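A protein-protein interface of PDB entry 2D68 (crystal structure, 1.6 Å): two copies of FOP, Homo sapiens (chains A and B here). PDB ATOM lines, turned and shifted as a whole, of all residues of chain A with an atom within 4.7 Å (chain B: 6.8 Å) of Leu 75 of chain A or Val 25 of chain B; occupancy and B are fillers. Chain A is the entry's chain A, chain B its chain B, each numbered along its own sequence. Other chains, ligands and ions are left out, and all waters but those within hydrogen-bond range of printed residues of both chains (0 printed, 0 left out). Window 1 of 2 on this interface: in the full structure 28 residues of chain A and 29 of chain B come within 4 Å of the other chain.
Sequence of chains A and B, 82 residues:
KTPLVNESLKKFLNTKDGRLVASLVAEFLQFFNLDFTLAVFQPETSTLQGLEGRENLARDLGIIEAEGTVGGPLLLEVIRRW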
ATOM      1  N   LEU A  24     -22.645   0.489 -31.033  1.00  0.00           N
ATOM      2  CA  LEU A  24     -23.890  -0.033 -30.452  1.00  0.00           C
ATOM      3  C   LEU A  24     -25.062   0.943 -30.580  1.00  0.00           C
ATOM      4  O   LEU A  24     -26.175   0.530 -30.867  1.00  0.00           O
ATOM      5  CB  LEU A  24     -23.679  -0.415 -28.993  1.00  0.00           C
ATOM      6  CG  LEU A  24     -23.007  -1.774 -28.836  1.00  0.00           C
ATOM      7  CD1 LEU A  24     -22.396  -1.904 -27.474  1.00  0.00           C
ATOM      8  CD2 LEU A  24     -24.028  -2.886 -29.082  1.00  0.00           C
ATOM      9  N   VAL A  25     -24.805   2.235 -30.372  1.00  0.00           N
ATOM     10  CA  VAL A  25     -25.845   3.262 -30.541  1.00  0.00           C
ATOM     11  C   VAL A  25     -26.310   3.295 -32.002  1.00  0.00           C
ATOM     12  O   VAL A  25     -27.514   3.227 -32.275  1.00  0.00           O
ATOM     13  CB  VAL A  25     -25.329   4.633 -30.051  1.00  0.00           C
ATOM     14  CG1 VAL A  25     -26.266   5.753 -30.481  1.00  0.00           C
ATOM     15  CG2 VAL A  25     -25.202   4.603 -28.526  1.00  0.00           C
ATOM     16  N   GLU A  27     -26.062   0.935 -34.234  1.00  0.00           N
ATOM     17  CA  GLU A  27     -26.764  -0.320 -34.566  1.00  0.00           C
ATOM     18  C   GLU A  27     -28.197  -0.296 -34.017  1.00  0.00           C
ATOM     19  O   GLU A  27     -29.112  -0.823 -34.646  1.00  0.00           O
ATOM     20  CB  GLU A  27     -25.999  -1.549 -34.069  1.00  0.00           C
ATOM     21  CG  GLU A  27     -26.470  -2.885 -34.661  1.00  0.00           C
ATOM     22  CD  GLU A  27     -27.637  -3.528 -33.910  1.00  0.00           C
ATOM     23  OE1 GLU A  27     -27.690  -3.410 -32.676  1.00  0.00           O
ATOM     24  OE2 GLU A  27     -28.484  -4.171 -34.571  1.00  0.00           O
ATOM     25  N   PHE A  28     -28.391   0.310 -32.846  1.00  0.00           N
ATOM     26  CA  PHE A  28     -29.741   0.441 -32.287  1.00  0.00           C
ATOM     27  C   PHE A  28     -30.620   1.271 -33.228  1.00  0.00           C
ATOM     28  O   PHE A  28     -31.754   0.898 -33.523  1.00  0.00           O
ATOM     29  CB  PHE A  28     -29.669   1.078 -30.886  1.00  0.00           C
ATOM     30  CG  PHE A  28     -31.007   1.452 -30.322  1.00  0.00           C
ATOM     31  CD1 PHE A  28     -31.716   0.559 -29.519  1.00  0.00           C
ATOM     32  CD2 PHE A  28     -31.567   2.703 -30.587  1.00  0.00           C
ATOM     33  CE1 PHE A  28     -32.979   0.914 -29.002  1.00  0.00           C
ATOM     34  CE2 PHE A  28     -32.817   3.060 -30.077  1.00  0.00           C
ATOM     35  CZ  PHE A  28     -33.516   2.185 -29.278  1.00  0.00           C
ATOM     36  N   PRO A  73     -32.024  -5.340 -30.996  1.00  0.00           N
ATOM     37  CA  PRO A  73     -30.727  -4.696 -31.218  1.00  0.00           C
ATOM     38  C   PRO A  73     -29.686  -5.372 -30.331  1.00  0.00           C
ATOM     39  O   PRO A  73     -30.049  -5.967 -29.311  1.00  0.00           O
ATOM     40  CB  PRO A  73     -30.972  -3.251 -30.753  1.00  0.00           C
ATOM     41  CG  PRO A  73     -32.021  -3.401 -29.681  1.00  0.00           C
ATOM     42  CD  PRO A  73     -32.955  -4.474 -30.243  1.00  0.00           C
ATOM     43  N   LEU A  74     -28.407  -5.290 -30.698  1.00  0.00           N
ATOM     44  CA  LEU A  74     -27.373  -5.953 -29.895  1.00  0.00           C
ATOM     45  C   LEU A  74     -27.336  -5.428 -28.451  1.00  0.00           C
ATOM     46  O   LEU A  74     -27.076  -6.188 -27.517  1.00  0.00           O
ATOM     47  CB  LEU A  74     -26.001  -5.834 -30.567  1.00  0.00           C
ATOM     48  CG  LEU A  74     -25.782  -6.621 -31.852  1.00  0.00           C
ATOM     49  CD1 LEU A  74     -24.376  -6.329 -32.317  1.00  0.00           C
ATOM     50  CD2 LEU A  74     -26.002  -8.127 -31.671  1.00  0.00           C
ATOM     51  N   LEU A  75     -27.622  -4.134 -28.252  1.00  0.00           N
ATOM     52  CA  LEU A  75     -27.655  -3.584 -26.903  1.00  0.00           C
ATOM     53  C   LEU A  75     -28.646  -4.321 -26.009  1.00  0.00           C
ATOM     54  O   LEU A  75     -28.467  -4.365 -24.795  1.00  0.00           O
ATOM     55  CB  LEU A  75     -27.962  -2.085 -26.950  1.00  0.00           C
ATOM     56  CG  LEU A  75     -27.367  -1.129 -25.923  1.00  0.00           C
ATOM     57  CD1 LEU A  75     -25.870  -1.340 -25.692  1.00  0.00           C
ATOM     58  CD2 LEU A  75     -27.592   0.274 -26.450  1.00  0.00           C
ATOM     59  N   LEU A  76     -29.698  -4.890 -26.606  1.00  0.00           N
ATOM     60  CA  LEU A  76     -30.666  -5.647 -25.808  1.00  0.00           C
ATOM     61  C   LEU A  76     -30.023  -6.884 -25.190  1.00  0.00           C
ATOM     62  O   LEU A  76     -30.327  -7.229 -24.062  1.00  0.00           O
ATOM     63  CB  LEU A  76     -31.895  -6.045 -26.610  1.00  0.00           C
ATOM     64  CG  LEU A  76     -32.975  -6.858 -25.876  1.00  0.00           C
ATOM     65  CD1 LEU A  76     -33.587  -6.132 -24.680  1.00  0.00           C
ATOM     66  CD2 LEU A  76     -34.095  -7.256 -26.841  1.00  0.00           C
ATOM     67  N   GLU A  77     -29.157  -7.560 -25.944  1.00  0.00           N
ATOM     68  CA  GLU A  77     -28.520  -8.761 -25.416  1.00  0.00           C
ATOM     69  C   GLU A  77     -27.622  -8.416 -24.227  1.00  0.00           C
ATOM     70  O   GLU A  77     -27.620  -9.105 -23.202  1.00  0.00           O
ATOM     71  CB  GLU A  77     -27.732  -9.468 -26.518  1.00  0.00           C
ATOM     72  CG  GLU A  77     -26.970 -10.694 -26.044  1.00  0.00           C
ATOM     73  CD  GLU A  77     -27.830 -11.938 -25.853  1.00  0.00           C
ATOM     74  OE1 GLU A  77     -29.088 -11.857 -25.823  1.00  0.00           O
ATOM     75  OE2 GLU A  77     -27.208 -13.016 -25.711  1.00  0.00           O
ATOM     76  N   VAL A  78     -26.903  -7.301 -24.349  1.00  0.00           N
ATOM     77  CA  VAL A  78     -26.063  -6.812 -23.255  1.00  0.00           C
ATOM     78  C   VAL A  78     -26.890  -6.536 -21.997  1.00  0.00           C
ATOM     79  O   VAL A  78     -26.572  -7.003 -20.905  1.00  0.00           O
ATOM     80  CB  VAL A  78     -25.287  -5.550 -23.681  1.00  0.00           C
ATOM     81  CG1 VAL A  78     -24.577  -4.923 -22.480  1.00  0.00           C
ATOM     82  CG2 VAL A  78     -24.292  -5.892 -24.821  1.00  0.00           C
ATOM     83  N   ILE A  79     -27.976  -5.784 -22.150  1.00  0.00           N
ATOM     84  CA  ILE A  79     -28.827  -5.440 -21.007  1.00  0.00           C
ATOM     85  C   ILE A  79     -29.564  -6.654 -20.403  1.00  0.00           C
ATOM     86  O   ILE A  79     -29.690  -6.789 -19.181  1.00  0.00           O
ATOM     87  CB  ILE A  79     -29.786  -4.278 -21.387  1.00  0.00           C
ATOM     88  CG1 ILE A  79     -29.002  -2.957 -21.510  1.00  0.00           C
ATOM     89  CG2 ILE A  79     -30.925  -4.151 -20.384  1.00  0.00           C
ATOM     90  CD1 ILE A  79     -28.000  -2.668 -20.351  1.00  0.00           C
ATOM     91  N   PHE B  12     -41.028  -2.817 -27.994  1.00  0.00           N
ATOM     92  CA  PHE B  12     -39.720  -2.838 -27.346  1.00  0.00           C
ATOM     93  C   PHE B  12     -39.700  -1.906 -26.147  1.00  0.00           C
ATOM     94  O   PHE B  12     -39.263  -2.300 -25.062  1.00  0.00           O
ATOM     95  CB  PHE B  12     -38.657  -2.437 -28.376  1.00  0.00           C
ATOM     96  CG  PHE B  12     -37.247  -2.407 -27.852  1.00  0.00           C
ATOM     97  CD1 PHE B  12     -36.495  -3.581 -27.759  1.00  0.00           C
ATOM     98  CD2 PHE B  12     -36.646  -1.196 -27.522  1.00  0.00           C
ATOM     99  CE1 PHE B  12     -35.166  -3.539 -27.316  1.00  0.00           C
ATOM    100  CE2 PHE B  12     -35.325  -1.147 -27.072  1.00  0.00           C
ATOM    101  CZ  PHE B  12     -34.581  -2.315 -26.986  1.00  0.00           C
ATOM    102  N   ASP B  17     -36.508  -4.094 -20.174  1.00  0.00           N
ATOM    103  CA  ASP B  17     -35.157  -4.084 -20.745  1.00  0.00           C
ATOM    104  C   ASP B  17     -35.066  -3.120 -21.923  1.00  0.00           C
ATOM    105  O   ASP B  17     -34.070  -2.402 -22.080  1.00  0.00           O
ATOM    106  CB  ASP B  17     -34.717  -5.485 -21.176  1.00  0.00           C
ATOM    107  CG  ASP B  17     -34.395  -6.388 -20.001  1.00  0.00           C
ATOM    108  OD1 ASP B  17     -34.353  -5.893 -18.859  1.00  0.00           O
ATOM    109  OD2 ASP B  17     -34.187  -7.602 -20.224  1.00  0.00           O
ATOM    110  N   LEU B  20     -34.940   0.442 -20.855  1.00  0.00           N
ATOM    111  CA  LEU B  20     -33.595   0.706 -20.332  1.00  0.00           C
ATOM    112  C   LEU B  20     -32.579   0.909 -21.469  1.00  0.00           C
ATOM    113  O   LEU B  20     -31.797   1.860 -21.444  1.00  0.00           O
ATOM    114  CB  LEU B  20     -33.162  -0.431 -19.401  1.00  0.00           C
ATOM    115  CG  LEU B  20     -31.791  -0.338 -18.775  1.00  0.00           C
ATOM    116  CD1 LEU B  20     -31.569   1.013 -18.083  1.00  0.00           C
ATOM    117  CD2 LEU B  20     -31.631  -1.498 -17.790  1.00  0.00           C
ATOM    118  N   VAL B  21     -32.601   0.026 -22.464  1.00  0.00           N
ATOM    119  CA  VAL B  21     -31.734   0.195 -23.650  1.00  0.00           C
ATOM    120  C   VAL B  21     -31.928   1.577 -24.290  1.00  0.00           C
ATOM    121  O   VAL B  21     -30.953   2.337 -24.510  1.00  0.00           O
ATOM    122  CB  VAL B  21     -32.011  -0.904 -24.700  1.00  0.00           C
ATOM    123  CG1 VAL B  21     -31.293  -0.594 -26.002  1.00  0.00           C
ATOM    124  CG2 VAL B  21     -31.536  -2.256 -24.171  1.00  0.00           C
ATOM    125  N   ALA B  22     -33.182   1.911 -24.591  1.00  0.00           N
ATOM    126  CA  ALA B  22     -33.453   3.185 -25.269  1.00  0.00           C
ATOM    127  C   ALA B  22     -33.053   4.390 -24.417  1.00  0.00           C
ATOM    128  O   ALA B  22     -32.473   5.348 -24.926  1.00  0.00           O
ATOM    129  CB  ALA B  22     -34.912   3.286 -25.699  1.00  0.00           C
ATOM    130  N   SER B  23     -33.325   4.315 -23.118  1.00  0.00           N
ATOM    131  CA  SER B  23     -32.897   5.368 -22.191  1.00  0.00           C
ATOM    132  C   SER B  23     -31.370   5.538 -22.187  1.00  0.00           C
ATOM    133  O   SER B  23     -30.866   6.665 -22.157  1.00  0.00           O
ATOM    134  CB  SER B  23     -33.402   5.058 -20.774  1.00  0.00           C
ATOM    135  OG  SER B  23     -34.816   5.014 -20.725  1.00  0.00           O
ATOM    136  N   LEU B  24     -30.635   4.425 -22.251  1.00  0.00           N
ATOM    137  CA  LEU B  24     -29.164   4.503 -22.319  1.00  0.00           C
ATOM    138  C   LEU B  24     -28.686   5.164 -23.608  1.00  0.00           C
ATOM    139  O   LEU B  24     -27.695   5.921 -23.605  1.00  0.00           O
ATOM    140  CB  LEU B  24     -28.533   3.116 -22.174  1.00  0.00           C
ATOM    141  CG  LEU B  24     -28.560   2.530 -20.764  1.00  0.00           C
ATOM    142  CD1 LEU B  24     -28.326   1.022 -20.836  1.00  0.00           C
ATOM    143  CD2 LEU B  24     -27.543   3.208 -19.831  1.00  0.00           C
ATOM    144  N   VAL B  25     -29.361   4.875 -24.716  1.00  0.00           N
ATOM    145  CA  VAL B  25     -29.049   5.543 -25.985  1.00  0.00           C
ATOM    146  C   VAL B  25     -29.305   7.059 -25.888  1.00  0.00           C
ATOM    147  O   VAL B  25     -28.422   7.858 -26.236  1.00  0.00           O
ATOM    148  CB  VAL B  25     -29.828   4.898 -27.145  1.00  0.00           C
ATOM    149  CG1 VAL B  25     -29.618   5.691 -28.470  1.00  0.00           C
ATOM    150  CG2 VAL B  25     -29.362   3.456 -27.346  1.00  0.00           C
ATOM    151  N   ALA B  26     -30.469   7.454 -25.376  1.00  0.00           N
ATOM    152  CA  ALA B  26     -30.757   8.885 -25.185  1.00  0.00           C
ATOM    153  C   ALA B  26     -29.721   9.552 -24.270  1.00  0.00           C
ATOM    154  O   ALA B  26     -29.293  10.683 -24.541  1.00  0.00           O
ATOM    155  CB  ALA B  26     -32.174   9.084 -24.665  1.00  0.00           C
ATOM    156  N   GLU B  27     -29.284   8.842 -23.221  1.00  0.00           N
ATOM    157  CA  GLU B  27     -28.307   9.414 -22.295  1.00  0.00           C
ATOM    158  C   GLU B  27     -26.966   9.619 -22.984  1.00  0.00           C
ATOM    159  O   GLU B  27     -26.289  10.594 -22.719  1.00  0.00           O
ATOM    160  CB  GLU B  27     -28.154   8.565 -21.025  1.00  0.00           C
ATOM    161  CG  GLU B  27     -27.438   9.327 -19.867  1.00  0.00           C
ATOM    162  CD  GLU B  27     -25.909   9.214 -19.883  1.00  0.00           C
ATOM    163  OE1 GLU B  27     -25.374   8.198 -20.362  1.00  0.00           O
ATOM    164  OE2 GLU B  27     -25.246  10.145 -19.389  1.00  0.00           O
ATOM    165  N   PHE B  28     -26.592   8.699 -23.868  1.00  0.00           N
ATOM    166  CA  PHE B  28     -25.389   8.876 -24.654  1.00  0.00           C
ATOM    167  C   PHE B  28     -25.481  10.160 -25.502  1.00  0.00           C
ATOM    168  O   PHE B  28     -24.543  10.957 -25.536  1.00  0.00           O
ATOM    169  CB  PHE B  28     -25.154   7.641 -25.539  1.00  0.00           C
ATOM    170  CG  PHE B  28     -24.077   7.840 -26.556  1.00  0.00           C
ATOM    171  CD1 PHE B  28     -22.763   7.496 -26.281  1.00  0.00           C
ATOM    172  CD2 PHE B  28     -24.372   8.366 -27.818  1.00  0.00           C
ATOM    173  CE1 PHE B  28     -21.764   7.713 -27.232  1.00  0.00           C
ATOM    174  CE2 PHE B  28     -23.375   8.570 -28.763  1.00  0.00           C
ATOM    175  CZ  PHE B  28     -22.072   8.241 -28.465  1.00  0.00           C
ATOM    176  N   LEU B  29     -26.620  10.362 -26.161  1.00  0.00           N
ATOM    177  CA  LEU B  29     -26.809  11.563 -26.984  1.00  0.00           C
ATOM    178  C   LEU B  29     -26.717  12.814 -26.128  1.00  0.00           C
ATOM    179  O   LEU B  29     -26.062  13.803 -26.504  1.00  0.00           O
ATOM    180  CB  LEU B  29     -28.149  11.505 -27.738  1.00  0.00           C
ATOM    181  CG  LEU B  29     -28.340  10.323 -28.684  1.00  0.00           C
ATOM    182  CD1 LEU B  29     -29.796  10.361 -29.229  1.00  0.00           C
ATOM    183  CD2 LEU B  29     -27.346  10.358 -29.838  1.00  0.00           C
ATOM    184  N   GLN B  30     -27.346  12.785 -24.957  1.00  0.00           N
ATOM    185  CA  GLN B  30     -27.304  13.948 -24.052  1.00  0.00           C
ATOM    186  C   GLN B  30     -25.901  14.201 -23.512  1.00  0.00           C
ATOM    187  O   GLN B  30     -25.426  15.358 -23.472  1.00  0.00           O
ATOM    188  CB  GLN B  30     -28.341  13.796 -22.942  1.00  0.00           C
ATOM    189  CG  GLN B  30     -29.752  13.739 -23.537  1.00  0.00           C
ATOM    190  CD  GLN B  30     -30.864  14.066 -22.569  1.00  0.00           C
ATOM    191  OE1 GLN B  30     -31.649  13.194 -22.208  1.00  0.00           O
ATOM    192  NE2 GLN B  30     -30.968  15.334 -22.182  1.00  0.00           N
ATOM    193  N   LEU B  38     -30.842  14.404 -30.797  1.00  0.00           N
ATOM    194  CA  LEU B  38     -31.922  14.218 -29.829  1.00  0.00           C
ATOM    195  C   LEU B  38     -33.248  14.817 -30.314  1.00  0.00           C
ATOM    196  O   LEU B  38     -34.304  14.224 -30.118  1.00  0.00           O
ATOM    197  CB  LEU B  38     -31.527  14.801 -28.468  1.00  0.00           C
ATOM    198  CG  LEU B  38     -32.437  14.467 -27.297  1.00  0.00           C
ATOM    199  CD1 LEU B  38     -32.376  12.958 -27.022  1.00  0.00           C
ATOM    200  CD2 LEU B  38     -31.956  15.258 -26.094  1.00  0.00           C
ATOM    201  N   PHE B  41     -34.501  12.227 -32.685  1.00  0.00           N
ATOM    202  CA  PHE B  41     -34.717  10.978 -31.922  1.00  0.00           C
ATOM    203  C   PHE B  41     -36.035  10.963 -31.149  1.00  0.00           C
ATOM    204  O   PHE B  41     -36.785   9.985 -31.192  1.00  0.00           O
ATOM    205  CB  PHE B  41     -33.548  10.772 -30.959  1.00  0.00           C
ATOM    206  CG  PHE B  41     -33.620   9.502 -30.135  1.00  0.00           C
ATOM    207  CD1 PHE B  41     -33.111   8.309 -30.629  1.00  0.00           C
ATOM    208  CD2 PHE B  41     -34.164   9.522 -28.848  1.00  0.00           C
ATOM    209  CE1 PHE B  41     -33.142   7.136 -29.857  1.00  0.00           C
ATOM    210  CE2 PHE B  41     -34.206   8.353 -28.074  1.00  0.00           C
ATOM    211  CZ  PHE B  41     -33.696   7.163 -28.582  1.00  0.00           C
ATOM    212  N   LEU B  51     -37.018   9.901 -21.951  1.00  0.00           N
ATOM    213  CA  LEU B  51     -36.868   8.614 -21.278  1.00  0.00           C
ATOM    214  C   LEU B  51     -36.272   8.819 -19.879  1.00  0.00           C
ATOM    215  O   LEU B  51     -36.107   9.962 -19.428  1.00  0.00           O
ATOM    216  CB  LEU B  51     -36.024   7.686 -22.146  1.00  0.00           C
ATOM    217  CG  LEU B  51     -36.715   7.314 -23.474  1.00  0.00           C
ATOM    218  CD1 LEU B  51     -35.715   6.805 -24.524  1.00  0.00           C
ATOM    219  CD2 LEU B  51     -37.829   6.300 -23.223  1.00  0.00           C
ATOM    220  N   LEU B  57     -31.178   5.425 -14.374  1.00  0.00           N
ATOM    221  CA  LEU B  57     -30.608   4.266 -15.047  1.00  0.00           C
ATOM    222  C   LEU B  57     -29.478   3.638 -14.241  1.00  0.00           C
ATOM    223  O   LEU B  57     -29.417   2.422 -14.132  1.00  0.00           O
ATOM    224  CB  LEU B  57     -30.084   4.675 -16.425  1.00  0.00           C
ATOM    225  CG  LEU B  57     -31.111   5.329 -17.333  1.00  0.00           C
ATOM    226  CD1 LEU B  57     -30.432   5.710 -18.628  1.00  0.00           C
ATOM    227  CD2 LEU B  57     -32.290   4.444 -17.624  1.00  0.00           C
ATOM    228  N   LEU B  75     -23.320   4.209 -20.849  1.00  0.00           N
ATOM    229  CA  LEU B  75     -23.013   3.048 -21.702  1.00  0.00           C
ATOM    230  C   LEU B  75     -21.531   2.713 -21.707  1.00  0.00           C
ATOM    231  O   LEU B  75     -21.145   1.569 -21.927  1.00  0.00           O
ATOM    232  CB  LEU B  75     -23.495   3.277 -23.136  1.00  0.00           C
ATOM    233  CG  LEU B  75     -24.956   2.948 -23.403  1.00  0.00           C
ATOM    234  CD1 LEU B  75     -25.379   3.395 -24.800  1.00  0.00           C
ATOM    235  CD2 LEU B  75     -25.225   1.438 -23.213  1.00  0.00           C
ATOM    236  N   VAL B  78     -21.231   0.409 -18.772  1.00  0.00           N
ATOM    237  CA  VAL B  78     -21.870  -0.856 -19.146  1.00  0.00           C
ATOM    238  C   VAL B  78     -20.912  -1.673 -20.011  1.00  0.00           C
ATOM    239  O   VAL B  78     -20.654  -2.853 -19.741  1.00  0.00           O
ATOM    240  CB  VAL B  78     -23.222  -0.618 -19.855  1.00  0.00           C
ATOM    241  CG1 VAL B  78     -23.768  -1.942 -20.357  1.00  0.00           C
ATOM    242  CG2 VAL B  78     -24.216   0.029 -18.885  1.00  0.00           C
ATOM    243  N   ILE B  79     -20.331  -1.048 -21.032  1.00  0.00           N
ATOM    244  CA  ILE B  79     -19.478  -1.797 -21.943  1.00  0.00           C
ATOM    245  C   ILE B  79     -18.132  -2.212 -21.306  1.00  0.00           C
ATOM    246  O   ILE B  79     -17.632  -3.310 -21.574  1.00  0.00           O
ATOM    247  CB  ILE B  79     -19.329  -1.065 -23.294  1.00  0.00           C
ATOM    248  CG1 ILE B  79     -20.660  -1.096 -24.069  1.00  0.00           C
ATOM    249  CG2 ILE B  79     -18.198  -1.655 -24.122  1.00  0.00           C
ATOM    250  CD1 ILE B  79     -21.295  -2.483 -24.215  1.00  0.00           C
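Leu 24 of chain A touches Ile 79 of chain B (CD1 to CD1, 3.5 Å).
Phe 28 of chain A touches Phe 12 of chain B.
Pro 73 of chain A touches Phe 12 of chain B.
Val 21 of chain B touches Leu 75 of chain A (CG1 to CB, 3.8 Å).
Leu 75 of chain A touches Val 25 of chain B.
Leu 75 of chain A touches Leu 75 of chain B (CD1 to CD2, 3.8 Å).
Leu 76 of chain A touches Asp 17 of chain B (CD1 to CB, 3.7 Å).
CG1 of Val 78 of chain A touches CG1 of Val 78 of chain B, at 3.7 Å.
Ile 79 of chain A touches Leu 20 of chain B.
Leu 24 of chain B touches Ile 79 of chain A (CD1 to CD1, 3.7 Å).
Of the printed residues of chain B, Pro 73 of chain A touches Phe 12 (3.8 Å).
Of chain B, only Val 21 (3.8 Å), Val 25 (3.7 Å) and Leu 75 (3.8 Å) come within 4 Å of Leu 75 of chain A.
Of the printed residues of chain B, Val 78 of chain A touches Val 78 (3.7 Å).
Val 25 of chain B touches three residues of chain A.
Printed residues of chain A within 4 Å of Phe 28 of chain B: Val 25 (3.9 Å).
Leu 51 of chain B touches none of the printed residues of chain A.
The nearest printed residue of chain A that does not touch Leu 20 of chain B is Leu 75 of chain A (6.7 Å).
Of the 20 printed residues of chain B, 11 touch a printed residue of chain A.
Among the printed residues, 20 pairs touch across the chains.
Val 25 of chain A touches its own counterpart, Val 25 of chain B.
Val 25 of chain A touches Phe 28 of chain B, and with the chains exchanged Phe 28 of chain A touches Val 25 of chain B.
Leu 75 of chain A touches its own counterpart, Leu 75 of chain B.
Val 78 of chain B touches its own counterpart, Val 78 of chain A.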
